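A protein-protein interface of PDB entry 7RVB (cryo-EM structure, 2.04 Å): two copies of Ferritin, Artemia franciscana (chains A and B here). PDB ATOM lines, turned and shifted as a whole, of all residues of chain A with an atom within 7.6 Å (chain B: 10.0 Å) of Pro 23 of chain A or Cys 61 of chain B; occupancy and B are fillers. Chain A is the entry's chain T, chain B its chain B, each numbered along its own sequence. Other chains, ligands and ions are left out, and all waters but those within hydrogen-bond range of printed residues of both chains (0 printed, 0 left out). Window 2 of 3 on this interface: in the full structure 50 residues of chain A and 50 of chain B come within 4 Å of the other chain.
The side-chain sulfur (SG) of Cys 61 of chain B is disulfide-bonded to the side-chain sulfur (SG) of Cys 22 of chain A (2.0 Å).
O of Cys 22 of chain A lies within hydrogen-bond range of NH1 of Arg 25 of chain A (2.7 Å).
Arg 59 of chain B touches Cys 22 of chain A (NH1 to CB, 3.6 Å).
Lys 62 of chain B touches Cys 22 of chain A (NZ to N, 3.9 Å).
SG of Cys 61 of chain B touches CD of Pro 23 of chain A, 3.8 Å away.
Leu 90 of chain A touches Ala 55 of chain B.
Leu 90 of chain A touches Ala 58 of chain B.
Arg 59 of chain B touches His 95 of chain A (CD to CE1, 3.6 Å).
Pro 23 of chain A touches just one residue of chain B: Cys 61 (3.8 Å).
Of the printed residues of chain A, Cys 61 of chain B touches Cys 22 (2.0 Å) and Pro 23 (3.8 Å).
Cys 22 of chain A touches just these residues of chain B: Arg 59, Cys 61 and Lys 62.
No residue of chain B comes within 4 Å of Ser 24 of chain A.
Of the printed residues of chain A, Lys 62 of chain B touches Cys 22 (3.9 Å).
Of the printed residues of chain A, Ala 58 of chain B touches Leu 90 (3.9 Å).
Of the printed residues of chain B, Leu 90 of chain A touches Ala 55 and Ala 58.
Of the printed residues of chain A, Ala 55 of chain B touches Leu 90.
Of the printed residues of chain B, His 95 of chain A touches Arg 59.
Gly 93 of chain A touches none of the printed residues of chain B.
His 26 of chain A touches none of the printed residues of chain B.
The nearest residue of chain A that does not touch Cys 61 of chain B is Ser 24 of chain A (4.5 Å).
Hydrophobic or aromatic side chains of chain A within 4 Å of the printed part of chain B: Pro 23, Leu 90 and His 95.
Printed residues of chain B that touch a printed residue of chain A: Ala 55, Ala 58, Arg 59, Cys 61 and Lys 62.
Hydrophobic or aromatic side chains of chain B within 4 Å of the printed part of chain A: Ala 58.
No position is printed for both chains.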
ATOM      1  N   CYS A  22      15.907 -26.495  -0.923  1.00  0.00           N
ATOM      2  CA  CYS A  22      16.530 -27.418  -1.863  1.00  0.00           C
ATOM      3  C   CYS A  22      16.717 -28.795  -1.244  1.00  0.00           C
ATOM      4  O   CYS A  22      17.432 -28.943  -0.257  1.00  0.00           O
ATOM      5  CB  CYS A  22      17.876 -26.875  -2.328  1.00  0.00           C
ATOM      6  SG  CYS A  22      18.455 -27.584  -3.870  1.00  0.00           S
ATOM      7  N   PRO A  23      16.074 -29.806  -1.825  1.00  0.00           N
ATOM      8  CA  PRO A  23      16.205 -31.164  -1.287  1.00  0.00           C
ATOM      9  C   PRO A  23      17.427 -31.892  -1.825  1.00  0.00           C
ATOM     10  O   PRO A  23      17.521 -33.118  -1.705  1.00  0.00           O
ATOM     11  CB  PRO A  23      14.908 -31.838  -1.741  1.00  0.00           C
ATOM     12  CG  PRO A  23      14.595 -31.166  -3.038  1.00  0.00           C
ATOM     13  CD  PRO A  23      15.100 -29.741  -2.929  1.00  0.00           C
ATOM     14  N   SER A  24      18.365 -31.158  -2.421  1.00  0.00           N
ATOM     15  CA  SER A  24      19.547 -31.765  -3.030  1.00  0.00           C
ATOM     16  C   SER A  24      20.769 -30.919  -2.704  1.00  0.00           C
ATOM     17  O   SER A  24      20.891 -29.788  -3.186  1.00  0.00           O
ATOM     18  CB  SER A  24      19.373 -31.912  -4.541  1.00  0.00           C
ATOM     19  OG  SER A  24      18.553 -33.026  -4.851  1.00  0.00           O
ATOM     20  N   ARG A  25      21.668 -31.467  -1.881  1.00  0.00           N
ATOM     21  CA  ARG A  25      22.963 -30.849  -1.620  1.00  0.00           C
ATOM     22  C   ARG A  25      24.072 -31.896  -1.538  1.00  0.00           C
ATOM     23  O   ARG A  25      25.126 -31.630  -0.946  1.00  0.00           O
ATOM     24  CB  ARG A  25      22.925 -30.007  -0.334  1.00  0.00           C
ATOM     25  CG  ARG A  25      22.853 -30.804   0.967  1.00  0.00           C
ATOM     26  CD  ARG A  25      21.437 -31.259   1.293  1.00  0.00           C
ATOM     27  NE  ARG A  25      20.646 -30.195   1.897  1.00  0.00           N
ATOM     28  CZ  ARG A  25      19.328 -30.090   1.787  1.00  0.00           C
ATOM     29  NH1 ARG A  25      18.620 -30.970   1.099  1.00  0.00           N
ATOM     30  NH2 ARG A  25      18.707 -29.076   2.381  1.00  0.00           N
ATOM     31  N   HIS A  26      23.869 -33.063  -2.141  1.00  0.00           N
ATOM     32  CA  HIS A  26      24.746 -34.214  -1.965  1.00  0.00           C
ATOM     33  C   HIS A  26      25.940 -34.138  -2.918  1.00  0.00           C
ATOM     34  O   HIS A  26      26.247 -33.090  -3.493  1.00  0.00           O
ATOM     35  CB  HIS A  26      23.949 -35.501  -2.152  1.00  0.00           C
ATOM     36  CG  HIS A  26      22.744 -35.342  -3.027  1.00  0.00           C
ATOM     37  ND1 HIS A  26      22.833 -35.137  -4.388  1.00  0.00           N
ATOM     38  CD2 HIS A  26      21.422 -35.355  -2.735  1.00  0.00           C
ATOM     39  CE1 HIS A  26      21.618 -35.033  -4.896  1.00  0.00           C
ATOM     40  NE2 HIS A  26      20.744 -35.161  -3.914  1.00  0.00           N
ATOM     41  N   LEU A  90      28.050 -24.040  -7.182  1.00  0.00           N
ATOM     42  CA  LEU A  90      26.687 -24.362  -7.596  1.00  0.00           C
ATOM     43  C   LEU A  90      26.651 -25.462  -8.652  1.00  0.00           C
ATOM     44  O   LEU A  90      25.708 -26.258  -8.680  1.00  0.00           O
ATOM     45  CB  LEU A  90      25.982 -23.113  -8.116  1.00  0.00           C
ATOM     46  CG  LEU A  90      25.617 -22.073  -7.059  1.00  0.00           C
ATOM     47  CD1 LEU A  90      25.279 -20.752  -7.714  1.00  0.00           C
ATOM     48  CD2 LEU A  90      24.469 -22.561  -6.205  1.00  0.00           C
ATOM     49  N   GLY A  93      26.577 -28.970  -7.248  1.00  0.00           N
ATOM     50  CA  GLY A  93      25.388 -29.324  -6.505  1.00  0.00           C
ATOM     51  C   GLY A  93      25.311 -28.824  -5.081  1.00  0.00           C
ATOM     52  O   GLY A  93      24.450 -29.293  -4.331  1.00  0.00           O
ATOM     53  N   HIS A  95      25.381 -25.556  -1.971  1.00  0.00           N
ATOM     54  CA  HIS A  95      24.707 -24.310  -1.636  1.00  0.00           C
ATOM     55  C   HIS A  95      25.736 -23.277  -1.199  1.00  0.00           C
ATOM     56  O   HIS A  95      26.797 -23.623  -0.675  1.00  0.00           O
ATOM     57  CB  HIS A  95      23.686 -24.501  -0.509  1.00  0.00           C
ATOM     58  CG  HIS A  95      22.531 -25.375  -0.876  1.00  0.00           C
ATOM     59  ND1 HIS A  95      22.339 -25.867  -2.148  1.00  0.00           N
ATOM     60  CD2 HIS A  95      21.505 -25.850  -0.132  1.00  0.00           C
ATOM     61  CE1 HIS A  95      21.246 -26.607  -2.172  1.00  0.00           C
ATOM     62  NE2 HIS A  95      20.721 -26.614  -0.961  1.00  0.00           N
ATOM     63  N   ALA B  55      22.168 -16.437  -6.286  1.00  0.00           N
ATOM     64  CA  ALA B  55      22.721 -17.739  -5.927  1.00  0.00           C
ATOM     65  C   ALA B  55      21.623 -18.737  -5.587  1.00  0.00           C
ATOM     66  O   ALA B  55      21.755 -19.932  -5.869  1.00  0.00           O
ATOM     67  CB  ALA B  55      23.693 -17.595  -4.760  1.00  0.00           C
ATOM     68  N   PHE B  56      20.539 -18.270  -4.966  1.00  0.00           N
ATOM     69  CA  PHE B  56      19.450 -19.169  -4.603  1.00  0.00           C
ATOM     70  C   PHE B  56      18.767 -19.743  -5.835  1.00  0.00           C
ATOM     71  O   PHE B  56      18.464 -20.938  -5.881  1.00  0.00           O
ATOM     72  CB  PHE B  56      18.436 -18.441  -3.724  1.00  0.00           C
ATOM     73  CG  PHE B  56      17.209 -19.248  -3.414  1.00  0.00           C
ATOM     74  CD1 PHE B  56      17.213 -20.168  -2.383  1.00  0.00           C
ATOM     75  CD2 PHE B  56      16.048 -19.082  -4.146  1.00  0.00           C
ATOM     76  CE1 PHE B  56      16.089 -20.907  -2.092  1.00  0.00           C
ATOM     77  CE2 PHE B  56      14.921 -19.820  -3.860  1.00  0.00           C
ATOM     78  CZ  PHE B  56      14.941 -20.733  -2.831  1.00  0.00           C
ATOM     79  N   TYR B  57      18.515 -18.915  -6.845  1.00  0.00           N
ATOM     80  CA  TYR B  57      17.745 -19.409  -7.980  1.00  0.00           C
ATOM     81  C   TYR B  57      18.586 -20.170  -8.997  1.00  0.00           C
ATOM     82  O   TYR B  57      18.029 -20.683  -9.970  1.00  0.00           O
ATOM     83  CB  TYR B  57      17.010 -18.254  -8.660  1.00  0.00           C
ATOM     84  CG  TYR B  57      15.709 -17.927  -7.973  1.00  0.00           C
ATOM     85  CD1 TYR B  57      14.673 -18.846  -7.941  1.00  0.00           C
ATOM     86  CD2 TYR B  57      15.527 -16.714  -7.329  1.00  0.00           C
ATOM     87  CE1 TYR B  57      13.490 -18.561  -7.304  1.00  0.00           C
ATOM     88  CE2 TYR B  57      14.347 -16.421  -6.689  1.00  0.00           C
ATOM     89  CZ  TYR B  57      13.332 -17.349  -6.679  1.00  0.00           C
ATOM     90  OH  TYR B  57      12.151 -17.062  -6.042  1.00  0.00           O
ATOM     91  N   ALA B  58      19.897 -20.267  -8.798  1.00  0.00           N
ATOM     92  CA  ALA B  58      20.766 -21.012  -9.698  1.00  0.00           C
ATOM     93  C   ALA B  58      21.070 -22.421  -9.208  1.00  0.00           C
ATOM     94  O   ALA B  58      21.852 -23.125  -9.851  1.00  0.00           O
ATOM     95  CB  ALA B  58      22.075 -20.252  -9.916  1.00  0.00           C
ATOM     96  N   ARG B  59      20.480 -22.850  -8.095  1.00  0.00           N
ATOM     97  CA  ARG B  59      20.712 -24.200  -7.598  1.00  0.00           C
ATOM     98  C   ARG B  59      20.168 -25.229  -8.581  1.00  0.00           C
ATOM     99  O   ARG B  59      19.225 -24.967  -9.330  1.00  0.00           O
ATOM    100  CB  ARG B  59      20.050 -24.390  -6.236  1.00  0.00           C
ATOM    101  CG  ARG B  59      20.647 -23.566  -5.121  1.00  0.00           C
ATOM    102  CD  ARG B  59      19.824 -23.702  -3.857  1.00  0.00           C
ATOM    103  NE  ARG B  59      20.325 -22.857  -2.782  1.00  0.00           N
ATOM    104  CZ  ARG B  59      19.783 -22.782  -1.575  1.00  0.00           C
ATOM    105  NH1 ARG B  59      18.717 -23.492  -1.251  1.00  0.00           N
ATOM    106  NH2 ARG B  59      20.326 -21.975  -0.669  1.00  0.00           N
ATOM    107  N   ASP B  60      20.774 -26.418  -8.573  1.00  0.00           N
ATOM    108  CA  ASP B  60      20.367 -27.456  -9.512  1.00  0.00           C
ATOM    109  C   ASP B  60      18.962 -27.973  -9.236  1.00  0.00           C
ATOM    110  O   ASP B  60      18.373 -28.617 -10.109  1.00  0.00           O
ATOM    111  CB  ASP B  60      21.364 -28.616  -9.492  1.00  0.00           C
ATOM    112  CG  ASP B  60      21.388 -29.348  -8.169  1.00  0.00           C
ATOM    113  OD1 ASP B  60      20.921 -28.786  -7.158  1.00  0.00           O
ATOM    114  OD2 ASP B  60      21.880 -30.493  -8.141  1.00  0.00           O
ATOM    115  N   CYS B  61      18.416 -27.714  -8.054  1.00  0.00           N
ATOM    116  CA  CYS B  61      17.047 -28.091  -7.738  1.00  0.00           C
ATOM    117  C   CYS B  61      16.051 -26.962  -7.970  1.00  0.00           C
ATOM    118  O   CYS B  61      14.856 -27.157  -7.737  1.00  0.00           O
ATOM    119  CB  CYS B  61      16.952 -28.560  -6.289  1.00  0.00           C
ATOM    120  SG  CYS B  61      16.910 -27.207  -5.123  1.00  0.00           S
ATOM    121  N   LYS B  62      16.510 -25.791  -8.408  1.00  0.00           N
ATOM    122  CA  LYS B  62      15.629 -24.681  -8.750  1.00  0.00           C
ATOM    123  C   LYS B  62      15.669 -24.378 -10.241  1.00  0.00           C
ATOM    124  O   LYS B  62      14.643 -24.474 -10.919  1.00  0.00           O
ATOM    125  CB  LYS B  62      16.021 -23.434  -7.947  1.00  0.00           C
ATOM    126  CG  LYS B  62      15.621 -23.454  -6.485  1.00  0.00           C
ATOM    127  CD  LYS B  62      14.218 -23.978  -6.288  1.00  0.00           C
ATOM    128  CE  LYS B  62      13.746 -23.736  -4.867  1.00  0.00           C
ATOM    129  NZ  LYS B  62      14.164 -24.828  -3.950  1.00  0.00           N
ATOM    130  N   ALA B  63      16.841 -24.031 -10.768  1.00  0.00           N
ATOM    131  CA  ALA B  63      17.084 -23.856 -12.199  1.00  0.00           C
ATOM    132  C   ALA B  63      16.044 -22.944 -12.855  1.00  0.00           C
ATOM    133  O   ALA B  63      15.300 -23.346 -13.749  1.00  0.00           O
ATOM    134  CB  ALA B  63      17.145 -25.213 -12.901  1.00  0.00           C
ATOM    135  N   ALA B  64      16.009 -21.698 -12.399  1.00  0.00           N
ATOM    136  CA  ALA B  64      15.126 -20.674 -12.955  1.00  0.00           C
ATOM    137  C   ALA B  64      15.998 -19.630 -13.645  1.00  0.00           C
ATOM    138  O   ALA B  64      16.595 -18.776 -12.987  1.00  0.00           O
ATOM    139  CB  ALA B  64      14.257 -20.054 -11.868  1.00  0.00           C
ATOM    140  N   TRP B 109      12.971 -18.239  -0.596  1.00  0.00           N
ATOM    141  CA  TRP B 109      11.664 -17.722  -0.970  1.00  0.00           C
ATOM    142  C   TRP B 109      10.779 -18.863  -1.445  1.00  0.00           C
ATOM    143  O   TRP B 109      11.232 -19.751  -2.172  1.00  0.00           O
ATOM    144  CB  TRP B 109      11.784 -16.648  -2.056  1.00  0.00           C
ATOM    145  CG  TRP B 109      12.513 -15.431  -1.586  1.00  0.00           C
ATOM    146  CD1 TRP B 109      11.963 -14.296  -1.068  1.00  0.00           C
ATOM    147  CD2 TRP B 109      13.930 -15.232  -1.573  1.00  0.00           C
ATOM    148  NE1 TRP B 109      12.949 -13.401  -0.740  1.00  0.00           N
ATOM    149  CE2 TRP B 109      14.166 -13.953  -1.040  1.00  0.00           C
ATOM    150  CE3 TRP B 109      15.021 -16.012  -1.963  1.00  0.00           C
ATOM    151  CZ2 TRP B 109      15.447 -13.435  -0.887  1.00  0.00           C
ATOM    152  CZ3 TRP B 109      16.290 -15.498  -1.810  1.00  0.00           C
ATOM    153  CH2 TRP B 109      16.494 -14.222  -1.277  1.00  0.00           C
ATOM    154  N   PHE B 112       7.824 -16.984  -6.589  1.00  0.00           N
ATOM    155  CA  PHE B 112       8.298 -15.749  -7.205  1.00  0.00           C
ATOM    156  C   PHE B 112       7.628 -14.515  -6.610  1.00  0.00           C
ATOM    157  O   PHE B 112       8.242 -13.439  -6.560  1.00  0.00           O
ATOM    158  CB  PHE B 112       8.070 -15.796  -8.715  1.00  0.00           C
ATOM    159  CG  PHE B 112       8.771 -16.930  -9.408  1.00  0.00           C
ATOM    160  CD1 PHE B 112       9.951 -17.446  -8.908  1.00  0.00           C
ATOM    161  CD2 PHE B 112       8.255 -17.469 -10.571  1.00  0.00           C
ATOM    162  CE1 PHE B 112      10.597 -18.482  -9.548  1.00  0.00           C
ATOM    163  CE2 PHE B 112       8.897 -18.506 -11.216  1.00  0.00           C
ATOM    164  CZ  PHE B 112      10.068 -19.012 -10.703  1.00  0.00           C
